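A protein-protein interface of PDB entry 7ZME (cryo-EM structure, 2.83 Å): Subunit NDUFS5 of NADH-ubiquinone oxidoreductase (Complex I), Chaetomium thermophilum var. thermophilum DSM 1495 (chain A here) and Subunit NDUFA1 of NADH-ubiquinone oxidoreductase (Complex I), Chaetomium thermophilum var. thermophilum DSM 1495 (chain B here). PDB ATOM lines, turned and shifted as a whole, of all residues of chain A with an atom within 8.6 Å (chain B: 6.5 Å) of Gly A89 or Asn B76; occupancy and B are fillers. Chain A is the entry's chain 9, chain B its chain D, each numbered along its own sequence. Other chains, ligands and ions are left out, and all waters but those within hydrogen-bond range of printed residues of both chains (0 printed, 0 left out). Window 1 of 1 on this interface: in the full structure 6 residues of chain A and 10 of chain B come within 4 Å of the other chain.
Arg A86 touches none of the printed residues of chain B. Gly A89 touches just these residues of chain B: Arg B55, Leu B56, Pro B70, Pro B71, Gly B72 and Asn B76. Of the printed residues of chain B, Leu A91 touches Leu B56. Printed residues of chain A within 4 Å of Arg B54: Leu A90. Of the printed residues of chain A, Pro B71 touches Gly A89 (3.4 Å) and Thr A97 (3.7 Å). Asn B76 touches two residues of chain A. The nearest residue of chain B that does not touch Gly A89 is Phe B73 (4.02 Å).
The side-chain amide nitrogen (ND2) of Asn B76 is in hydrogen-bond range of the backbone carbonyl oxygen (O) of Leu A88 (3.3 Å). O of Gly A89 sits close to O of Arg B55 (2.9 Å).
The backbone carbonyl oxygen of Arg B55 sits at hydrogen-bond distance from the side-chain amide nitrogen of Asn B76, 2.9 Å away. The backbone NH (N) of Gly A89 is in hydrogen-bond range of the side-chain hydroxyl (OG1) of Thr A97 (3.1 Å). The guanidinium group of Arg B55 sits at hydrogen-bond distance from the side-chain amide oxygen of Asn B77 (3.2 Å). The guanidinium group (NH2) of Arg B55 is in hydrogen-bond range of the backbone carbonyl oxygen (O) of Phe B73, 2.8 Å away. O of Phe B73 sits close to OD1 of Asn B76 (2.7 Å).
Among the printed residues, merely in contact across the chains: His A101 with Phe B75, Gly A89 with Pro B70, Leu A90 with Pro B70, Gly A89 with Pro B71, Gly A89 with Asn B76, Leu A90 with Gly B58, Leu A88 with Gly B72, Leu A90 with Thr B57, Thr A97 with Pro B71, Leu A88 with Phe B75, Gly A89 with Leu B56, Gly A89 with Gly B72, Leu A91 with Leu B56 and Leu A90 with Arg B54.
Hydrophobic or aromatic side chains of chain B that line the printed part of chain A: Pro B70 and Phe B75. Hydrophobic or aromatic side chains of chain A that line the printed part of chain B: Leu A88, Leu A90 and His A101.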
ATOM      1  N   GLN A  84     -24.755  20.199  24.777  1.00  0.00           N
ATOM      2  CA  GLN A  84     -24.086  19.887  26.067  1.00  0.00           C
ATOM      3  C   GLN A  84     -24.803  18.716  26.739  1.00  0.00           C
ATOM      4  O   GLN A  84     -24.117  17.872  27.344  1.00  0.00           O
ATOM      5  CB  GLN A  84     -24.063  21.118  26.972  1.00  0.00           C
ATOM      6  CG  GLN A  84     -22.894  22.051  26.697  1.00  0.00           C
ATOM      7  CD  GLN A  84     -22.987  23.327  27.496  1.00  0.00           C
ATOM      8  OE1 GLN A  84     -23.966  23.573  28.196  1.00  0.00           O
ATOM      9  NE2 GLN A  84     -21.960  24.154  27.394  1.00  0.00           N
ATOM     10  N   ILE A  85     -26.125  18.656  26.615  1.00  0.00           N
ATOM     11  CA  ILE A  85     -26.899  17.514  27.172  1.00  0.00           C
ATOM     12  C   ILE A  85     -26.465  16.239  26.444  1.00  0.00           C
ATOM     13  O   ILE A  85     -26.332  15.198  27.110  1.00  0.00           O
ATOM     14  CB  ILE A  85     -28.407  17.783  27.040  1.00  0.00           C
ATOM     15  CG1 ILE A  85     -28.776  19.197  27.496  1.00  0.00           C
ATOM     16  CG2 ILE A  85     -29.214  16.729  27.782  1.00  0.00           C
ATOM     17  CD1 ILE A  85     -28.538  19.449  28.965  1.00  0.00           C
ATOM     18  N   ARG A  86     -26.235  16.322  25.134  1.00  0.00           N
ATOM     19  CA  ARG A  86     -25.806  15.154  24.319  1.00  0.00           C
ATOM     20  C   ARG A  86     -24.453  14.652  24.816  1.00  0.00           C
ATOM     21  O   ARG A  86     -24.210  13.441  24.735  1.00  0.00           O
ATOM     22  CB  ARG A  86     -25.660  15.558  22.848  1.00  0.00           C
ATOM     23  CG  ARG A  86     -26.845  15.208  21.961  1.00  0.00           C
ATOM     24  CD  ARG A  86     -28.033  16.100  22.248  1.00  0.00           C
ATOM     25  NE  ARG A  86     -29.080  16.055  21.240  1.00  0.00           N
ATOM     26  CZ  ARG A  86     -29.246  16.969  20.293  1.00  0.00           C
ATOM     27  NH1 ARG A  86     -28.427  18.004  20.223  1.00  0.00           N
ATOM     28  NH2 ARG A  86     -30.232  16.848  19.423  1.00  0.00           N
ATOM     29  N   ASN A  87     -23.586  15.560  25.251  1.00  0.00           N
ATOM     30  CA  ASN A  87     -22.208  15.199  25.665  1.00  0.00           C
ATOM     31  C   ASN A  87     -22.164  14.460  27.006  1.00  0.00           C
ATOM     32  O   ASN A  87     -21.097  13.911  27.323  1.00  0.00           O
ATOM     33  CB  ASN A  87     -21.289  16.415  25.604  1.00  0.00           C
ATOM     34  CG  ASN A  87     -21.137  16.942  24.193  1.00  0.00           C
ATOM     35  OD1 ASN A  87     -21.033  16.166  23.245  1.00  0.00           O
ATOM     36  ND2 ASN A  87     -21.129  18.255  24.041  1.00  0.00           N
ATOM     37  N   LEU A  88     -23.245  14.463  27.778  1.00  0.00           N
ATOM     38  CA  LEU A  88     -23.172  13.829  29.117  1.00  0.00           C
ATOM     39  C   LEU A  88     -22.850  12.336  28.971  1.00  0.00           C
ATOM     40  O   LEU A  88     -23.467  11.692  28.104  1.00  0.00           O
ATOM     41  CB  LEU A  88     -24.523  14.049  29.801  1.00  0.00           C
ATOM     42  CG  LEU A  88     -24.694  13.495  31.212  1.00  0.00           C
ATOM     43  CD1 LEU A  88     -24.216  14.508  32.234  1.00  0.00           C
ATOM     44  CD2 LEU A  88     -26.155  13.172  31.470  1.00  0.00           C
ATOM     45  N   GLY A  89     -21.911  11.811  29.766  1.00  0.00           N
ATOM     46  CA  GLY A  89     -21.620  10.366  29.776  1.00  0.00           C
ATOM     47  C   GLY A  89     -20.798   9.887  28.593  1.00  0.00           C
ATOM     48  O   GLY A  89     -20.998   8.736  28.171  1.00  0.00           O
ATOM     49  N   LEU A  90     -19.917  10.727  28.050  1.00  0.00           N
ATOM     50  CA  LEU A  90     -19.191  10.266  26.879  1.00  0.00           C
ATOM     51  C   LEU A  90     -17.752   9.929  27.258  1.00  0.00           C
ATOM     52  O   LEU A  90     -17.328  10.096  28.405  1.00  0.00           O
ATOM     53  CB  LEU A  90     -19.250  11.308  25.761  1.00  0.00           C
ATOM     54  CG  LEU A  90     -20.628  11.517  25.127  1.00  0.00           C
ATOM     55  CD1 LEU A  90     -20.536  12.488  23.960  1.00  0.00           C
ATOM     56  CD2 LEU A  90     -21.229  10.195  24.681  1.00  0.00           C
ATOM     57  N   LEU A  91     -17.000   9.442  26.269  1.00  0.00           N
ATOM     58  CA  LEU A  91     -15.658   8.931  26.529  1.00  0.00           C
ATOM     59  C   LEU A  91     -14.707  10.039  26.971  1.00  0.00           C
ATOM     60  O   LEU A  91     -13.973   9.883  27.954  1.00  0.00           O
ATOM     61  CB  LEU A  91     -15.119   8.226  25.285  1.00  0.00           C
ATOM     62  CG  LEU A  91     -13.973   7.236  25.501  1.00  0.00           C
ATOM     63  CD1 LEU A  91     -14.297   6.270  26.630  1.00  0.00           C
ATOM     64  CD2 LEU A  91     -13.668   6.482  24.215  1.00  0.00           C
ATOM     65  N   ASN A  92     -14.701  11.164  26.260  1.00  0.00           N
ATOM     66  CA  ASN A  92     -13.711  12.211  26.499  1.00  0.00           C
ATOM     67  C   ASN A  92     -14.365  13.585  26.514  1.00  0.00           C
ATOM     68  O   ASN A  92     -13.852  14.542  25.926  1.00  0.00           O
ATOM     69  CB  ASN A  92     -12.597  12.161  25.455  1.00  0.00           C
ATOM     70  CG  ASN A  92     -11.299  12.756  25.959  1.00  0.00           C
ATOM     71  OD1 ASN A  92     -11.206  13.188  27.109  1.00  0.00           O
ATOM     72  ND2 ASN A  92     -10.287  12.786  25.100  1.00  0.00           N
ATOM     73  N   LYS A  93     -15.504  13.703  27.191  1.00  0.00           N
ATOM     74  CA  LYS A  93     -16.224  14.966  27.322  1.00  0.00           C
ATOM     75  C   LYS A  93     -16.496  15.268  28.790  1.00  0.00           C
ATOM     76  O   LYS A  93     -17.616  15.589  29.192  1.00  0.00           O
ATOM     77  CB  LYS A  93     -17.523  14.944  26.520  1.00  0.00           C
ATOM     78  CG  LYS A  93     -17.342  14.607  25.049  1.00  0.00           C
ATOM     79  CD  LYS A  93     -16.453  15.628  24.356  1.00  0.00           C
ATOM     80  CE  LYS A  93     -17.223  16.888  24.000  1.00  0.00           C
ATOM     81  NZ  LYS A  93     -16.379  17.858  23.248  1.00  0.00           N
ATOM     82  N   GLU A  94     -15.453  15.158  29.618  1.00  0.00           N
ATOM     83  CA  GLU A  94     -15.615  15.371  31.052  1.00  0.00           C
ATOM     84  C   GLU A  94     -16.034  16.800  31.371  1.00  0.00           C
ATOM     85  O   GLU A  94     -16.730  17.033  32.366  1.00  0.00           O
ATOM     86  CB  GLU A  94     -14.317  15.030  31.784  1.00  0.00           C
ATOM     87  CG  GLU A  94     -13.975  13.549  31.793  1.00  0.00           C
ATOM     88  CD  GLU A  94     -12.817  13.214  30.872  1.00  0.00           C
ATOM     89  OE1 GLU A  94     -12.434  14.079  30.056  1.00  0.00           O
ATOM     90  OE2 GLU A  94     -12.287  12.086  30.965  1.00  0.00           O
ATOM     91  N   ASP A  96     -18.104  18.808  29.680  1.00  0.00           N
ATOM     92  CA  ASP A  96     -19.523  19.057  29.454  1.00  0.00           C
ATOM     93  C   ASP A  96     -20.386  18.381  30.511  1.00  0.00           C
ATOM     94  O   ASP A  96     -21.351  18.976  31.004  1.00  0.00           O
ATOM     95  CB  ASP A  96     -19.919  18.592  28.056  1.00  0.00           C
ATOM     96  CG  ASP A  96     -19.401  19.513  26.969  1.00  0.00           C
ATOM     97  OD1 ASP A  96     -19.232  20.719  27.242  1.00  0.00           O
ATOM     98  OD2 ASP A  96     -19.163  19.030  25.842  1.00  0.00           O
ATOM     99  N   THR A  97     -20.061  17.134  30.865  1.00  0.00           N
ATOM    100  CA  THR A  97     -20.819  16.429  31.895  1.00  0.00           C
ATOM    101  C   THR A  97     -20.818  17.203  33.206  1.00  0.00           C
ATOM    102  O   THR A  97     -21.841  17.268  33.899  1.00  0.00           O
ATOM    103  CB  THR A  97     -20.246  15.024  32.094  1.00  0.00           C
ATOM    104  OG1 THR A  97     -20.403  14.264  30.889  1.00  0.00           O
ATOM    105  CG2 THR A  97     -20.939  14.303  33.237  1.00  0.00           C
ATOM    106  N   LYS A  98     -19.680  17.806  33.560  1.00  0.00           N
ATOM    107  CA  LYS A  98     -19.613  18.602  34.782  1.00  0.00           C
ATOM    108  C   LYS A  98     -20.512  19.830  34.694  1.00  0.00           C
ATOM    109  O   LYS A  98     -21.168  20.199  35.675  1.00  0.00           O
ATOM    110  CB  LYS A  98     -18.168  19.011  35.062  1.00  0.00           C
ATOM    111  CG  LYS A  98     -17.309  17.892  35.626  1.00  0.00           C
ATOM    112  CD  LYS A  98     -15.975  18.418  36.129  1.00  0.00           C
ATOM    113  CE  LYS A  98     -16.131  19.125  37.465  1.00  0.00           C
ATOM    114  NZ  LYS A  98     -16.394  18.166  38.572  1.00  0.00           N
ATOM    115  N   VAL A 100     -23.266  20.152  32.993  1.00  0.00           N
ATOM    116  CA  VAL A 100     -24.648  19.701  33.116  1.00  0.00           C
ATOM    117  C   VAL A 100     -25.084  19.543  34.564  1.00  0.00           C
ATOM    118  O   VAL A 100     -26.255  19.773  34.881  1.00  0.00           O
ATOM    119  CB  VAL A 100     -24.833  18.373  32.352  1.00  0.00           C
ATOM    120  CG1 VAL A 100     -26.227  17.802  32.566  1.00  0.00           C
ATOM    121  CG2 VAL A 100     -24.567  18.572  30.870  1.00  0.00           C
ATOM    122  N   HIS A 101     -24.163  19.191  35.458  1.00  0.00           N
ATOM    123  CA  HIS A 101     -24.491  18.916  36.850  1.00  0.00           C
ATOM    124  C   HIS A 101     -24.197  20.093  37.769  1.00  0.00           C
ATOM    125  O   HIS A 101     -24.317  19.954  38.992  1.00  0.00           O
ATOM    126  CB  HIS A 101     -23.731  17.679  37.325  1.00  0.00           C
ATOM    127  CG  HIS A 101     -24.210  16.407  36.702  1.00  0.00           C
ATOM    128  ND1 HIS A 101     -25.406  16.316  36.026  1.00  0.00           N
ATOM    129  CD2 HIS A 101     -23.651  15.176  36.645  1.00  0.00           C
ATOM    130  CE1 HIS A 101     -25.566  15.083  35.583  1.00  0.00           C
ATOM    131  NE2 HIS A 101     -24.515  14.372  35.945  1.00  0.00           N
ATOM    132  N   ARG B  54     -25.132   4.667  22.106  1.00  0.00           N
ATOM    133  CA  ARG B  54     -25.091   6.147  21.983  1.00  0.00           C
ATOM    134  C   ARG B  54     -24.839   6.729  23.373  1.00  0.00           C
ATOM    135  O   ARG B  54     -24.132   7.733  23.471  1.00  0.00           O
ATOM    136  CB  ARG B  54     -26.379   6.661  21.335  1.00  0.00           C
ATOM    137  CG  ARG B  54     -26.320   8.112  20.887  1.00  0.00           C
ATOM    138  CD  ARG B  54     -27.627   8.867  21.000  1.00  0.00           C
ATOM    139  NE  ARG B  54     -28.465   8.843  19.810  1.00  0.00           N
ATOM    140  CZ  ARG B  54     -29.679   8.315  19.759  1.00  0.00           C
ATOM    141  NH1 ARG B  54     -30.370   8.356  18.633  1.00  0.00           N
ATOM    142  NH2 ARG B  54     -30.200   7.753  20.833  1.00  0.00           N
ATOM    143  N   ARG B  55     -25.392   6.105  24.412  1.00  0.00           N
ATOM    144  CA  ARG B  55     -25.173   6.551  25.808  1.00  0.00           C
ATOM    145  C   ARG B  55     -23.682   6.491  26.167  1.00  0.00           C
ATOM    146  O   ARG B  55     -23.249   7.340  26.958  1.00  0.00           O
ATOM    147  CB  ARG B  55     -26.037   5.732  26.765  1.00  0.00           C
ATOM    148  CG  ARG B  55     -27.519   6.062  26.734  1.00  0.00           C
ATOM    149  CD  ARG B  55     -28.240   5.110  27.662  1.00  0.00           C
ATOM    150  NE  ARG B  55     -27.826   5.292  29.043  1.00  0.00           N
ATOM    151  CZ  ARG B  55     -28.066   4.425  30.016  1.00  0.00           C
ATOM    152  NH1 ARG B  55     -28.706   3.299  29.753  1.00  0.00           N
ATOM    153  NH2 ARG B  55     -27.658   4.680  31.245  1.00  0.00           N
ATOM    154  N   LEU B  56     -22.935   5.512  25.654  1.00  0.00           N
ATOM    155  CA  LEU B  56     -21.500   5.360  26.017  1.00  0.00           C
ATOM    156  C   LEU B  56     -20.579   6.034  24.990  1.00  0.00           C
ATOM    157  O   LEU B  56     -19.524   6.511  25.408  1.00  0.00           O
ATOM    158  CB  LEU B  56     -21.190   3.863  26.107  1.00  0.00           C
ATOM    159  CG  LEU B  56     -21.849   3.093  27.248  1.00  0.00           C
ATOM    160  CD1 LEU B  56     -22.215   1.684  26.816  1.00  0.00           C
ATOM    161  CD2 LEU B  56     -20.946   3.057  28.468  1.00  0.00           C
ATOM    162  N   THR B  57     -20.948   6.095  23.708  1.00  0.00           N
ATOM    163  CA  THR B  57     -20.046   6.620  22.693  1.00  0.00           C
ATOM    164  C   THR B  57     -20.588   7.813  21.924  1.00  0.00           C
ATOM    165  O   THR B  57     -19.800   8.506  21.273  1.00  0.00           O
ATOM    166  CB  THR B  57     -19.676   5.526  21.674  1.00  0.00           C
ATOM    167  OG1 THR B  57     -20.766   5.323  20.769  1.00  0.00           O
ATOM    168  CG2 THR B  57     -19.343   4.211  22.372  1.00  0.00           C
ATOM    169  N   GLY B  58     -21.893   8.069  21.967  1.00  0.00           N
ATOM    170  CA  GLY B  58     -22.496   9.142  21.213  1.00  0.00           C
ATOM    171  C   GLY B  58     -23.014   8.741  19.850  1.00  0.00           C
ATOM    172  O   GLY B  58     -23.887   9.422  19.305  1.00  0.00           O
ATOM    173  N   PRO B  70     -18.324   5.627  31.704  1.00  0.00           N
ATOM    174  CA  PRO B  70     -17.876   6.994  31.910  1.00  0.00           C
ATOM    175  C   PRO B  70     -18.827   7.754  32.841  1.00  0.00           C
ATOM    176  O   PRO B  70     -19.985   7.437  32.881  1.00  0.00           O
ATOM    177  CB  PRO B  70     -17.953   7.618  30.520  1.00  0.00           C
ATOM    178  CG  PRO B  70     -19.023   6.851  29.817  1.00  0.00           C
ATOM    179  CD  PRO B  70     -18.767   5.447  30.297  1.00  0.00           C
ATOM    180  N   PRO B  71     -18.354   8.761  33.599  1.00  0.00           N
ATOM    181  CA  PRO B  71     -19.207   9.462  34.557  1.00  0.00           C
ATOM    182  C   PRO B  71     -20.373  10.163  33.846  1.00  0.00           C
ATOM    183  O   PRO B  71     -20.158  10.691  32.778  1.00  0.00           O
ATOM    184  CB  PRO B  71     -18.259  10.473  35.220  1.00  0.00           C
ATOM    185  CG  PRO B  71     -17.108  10.617  34.248  1.00  0.00           C
ATOM    186  CD  PRO B  71     -16.976   9.256  33.600  1.00  0.00           C
ATOM    187  N   GLY B  72     -21.560  10.169  34.459  1.00  0.00           N
ATOM    188  CA  GLY B  72     -22.756  10.756  33.822  1.00  0.00           C
ATOM    189  C   GLY B  72     -23.571   9.718  33.085  1.00  0.00           C
ATOM    190  O   GLY B  72     -24.639  10.085  32.604  1.00  0.00           O
ATOM    191  N   PHE B  73     -23.089   8.472  33.009  1.00  0.00           N
ATOM    192  CA  PHE B  73     -23.804   7.356  32.331  1.00  0.00           C
ATOM    193  C   PHE B  73     -25.098   7.065  33.087  1.00  0.00           C
ATOM    194  O   PHE B  73     -26.098   6.723  32.454  1.00  0.00           O
ATOM    195  CB  PHE B  73     -22.908   6.134  32.156  1.00  0.00           C
ATOM    196  CG  PHE B  73     -23.548   4.978  31.434  1.00  0.00           C
ATOM    197  CD1 PHE B  73     -23.770   5.029  30.069  1.00  0.00           C
ATOM    198  CD2 PHE B  73     -23.924   3.836  32.121  1.00  0.00           C
ATOM    199  CE1 PHE B  73     -24.363   3.966  29.408  1.00  0.00           C
ATOM    200  CE2 PHE B  73     -24.512   2.774  31.456  1.00  0.00           C
ATOM    201  CZ  PHE B  73     -24.730   2.842  30.102  1.00  0.00           C
ATOM    202  N   GLU B  74     -25.208   7.162  34.305  1.00  0.00           N
ATOM    203  CA  GLU B  74     -26.400   6.807  35.110  1.00  0.00           C
ATOM    204  C   GLU B  74     -27.477   7.889  35.002  1.00  0.00           C
ATOM    205  O   GLU B  74     -28.617   7.605  35.350  1.00  0.00           O
ATOM    206  CB  GLU B  74     -25.857   6.755  36.532  1.00  0.00           C
ATOM    207  CG  GLU B  74     -24.588   7.571  36.668  1.00  0.00           C
ATOM    208  CD  GLU B  74     -24.187   7.944  38.081  1.00  0.00           C
ATOM    209  OE1 GLU B  74     -23.013   8.302  38.278  1.00  0.00           O
ATOM    210  OE2 GLU B  74     -25.052   7.889  38.975  1.00  0.00           O
ATOM    211  N   PHE B  75     -27.044   9.149  34.610  1.00  0.00           N
ATOM    212  CA  PHE B  75     -28.017  10.239  34.362  1.00  0.00           C
ATOM    213  C   PHE B  75     -28.348  10.399  32.876  1.00  0.00           C
ATOM    214  O   PHE B  75     -29.252  11.190  32.588  1.00  0.00           O
ATOM    215  CB  PHE B  75     -27.403  11.554  34.835  1.00  0.00           C
ATOM    216  CG  PHE B  75     -26.799  11.524  36.214  1.00  0.00           C
ATOM    217  CD1 PHE B  75     -27.596  11.649  37.338  1.00  0.00           C
ATOM    218  CD2 PHE B  75     -25.433  11.387  36.386  1.00  0.00           C
ATOM    219  CE1 PHE B  75     -27.039  11.632  38.604  1.00  0.00           C
ATOM    220  CE2 PHE B  75     -24.877  11.379  37.654  1.00  0.00           C
ATOM    221  CZ  PHE B  75     -25.681  11.498  38.761  1.00  0.00           C
ATOM    222  N   ASN B  76     -27.693   9.669  31.967  1.00  0.00           N
ATOM    223  CA  ASN B  76     -27.900   9.899  30.505  1.00  0.00           C
ATOM    224  C   ASN B  76     -28.929   8.933  29.922  1.00  0.00           C
ATOM    225  O   ASN B  76     -29.015   8.865  28.694  1.00  0.00           O
ATOM    226  CB  ASN B  76     -26.593   9.958  29.698  1.00  0.00           C
ATOM    227  CG  ASN B  76     -25.836   8.655  29.563  1.00  0.00           C
ATOM    228  OD1 ASN B  76     -26.336   7.587  29.892  1.00  0.00           O
ATOM    229  ND2 ASN B  76     -24.621   8.733  29.051  1.00  0.00           N
ATOM    230  N   ASN B  77     -29.693   8.241  30.767  1.00  0.00           N
ATOM    231  CA  ASN B  77     -30.626   7.209  30.247  1.00  0.00           C
ATOM    232  C   ASN B  77     -31.821   7.948  29.645  1.00  0.00           C
ATOM    233  O   ASN B  77     -32.480   8.698  30.377  1.00  0.00           O
ATOM    234  CB  ASN B  77     -31.054   6.191  31.300  1.00  0.00           C
ATOM    235  CG  ASN B  77     -31.740   4.974  30.723  1.00  0.00           C
ATOM    236  OD1 ASN B  77     -31.629   4.693  29.534  1.00  0.00           O
ATOM    237  ND2 ASN B  77     -32.438   4.232  31.565  1.00  0.00           N
ATOM    238  N   PRO B  78     -32.087   7.853  28.322  1.00  0.00           N
ATOM    239  CA  PRO B  78     -33.157   8.635  27.697  1.00  0.00           C
ATOM    240  C   PRO B  78     -34.516   8.036  28.017  1.00  0.00           C
ATOM    241  O   PRO B  78     -34.721   6.827  27.896  1.00  0.00           O
ATOM    242  CB  PRO B  78     -32.841   8.537  26.198  1.00  0.00           C
ATOM    243  CG  PRO B  78     -31.501   7.854  26.107  1.00  0.00           C
ATOM    244  CD  PRO B  78     -31.395   7.018  27.335  1.00  0.00           C
ATOM    245  N   TRP B  79     -35.441   8.886  28.435  1.00  0.00           N
ATOM    246  CA  TRP B  79     -36.833   8.502  28.595  1.00  0.00           C
ATOM    247  C   TRP B  79     -37.631   9.196  27.502  1.00  0.00           C
ATOM    248  O   TRP B  79     -37.667  10.428  27.443  1.00  0.00           O
ATOM    249  CB  TRP B  79     -37.347   8.863  29.987  1.00  0.00           C
ATOM    250  CG  TRP B  79     -37.032   7.814  31.000  1.00  0.00           C
ATOM    251  CD1 TRP B  79     -36.098   6.835  30.889  1.00  0.00           C
ATOM    252  CD2 TRP B  79     -37.653   7.633  32.276  1.00  0.00           C
ATOM    253  NE1 TRP B  79     -36.092   6.054  32.012  1.00  0.00           N
ATOM    254  CE2 TRP B  79     -37.038   6.524  32.883  1.00  0.00           C
ATOM    255  CE3 TRP B  79     -38.670   8.303  32.965  1.00  0.00           C
ATOM    256  CZ2 TRP B  79     -37.404   6.067  34.142  1.00  0.00           C
ATOM    257  CZ3 TRP B  79     -39.031   7.847  34.216  1.00  0.00           C
ATOM    258  CH2 TRP B  79     -38.399   6.739  34.791  1.00  0.00           C
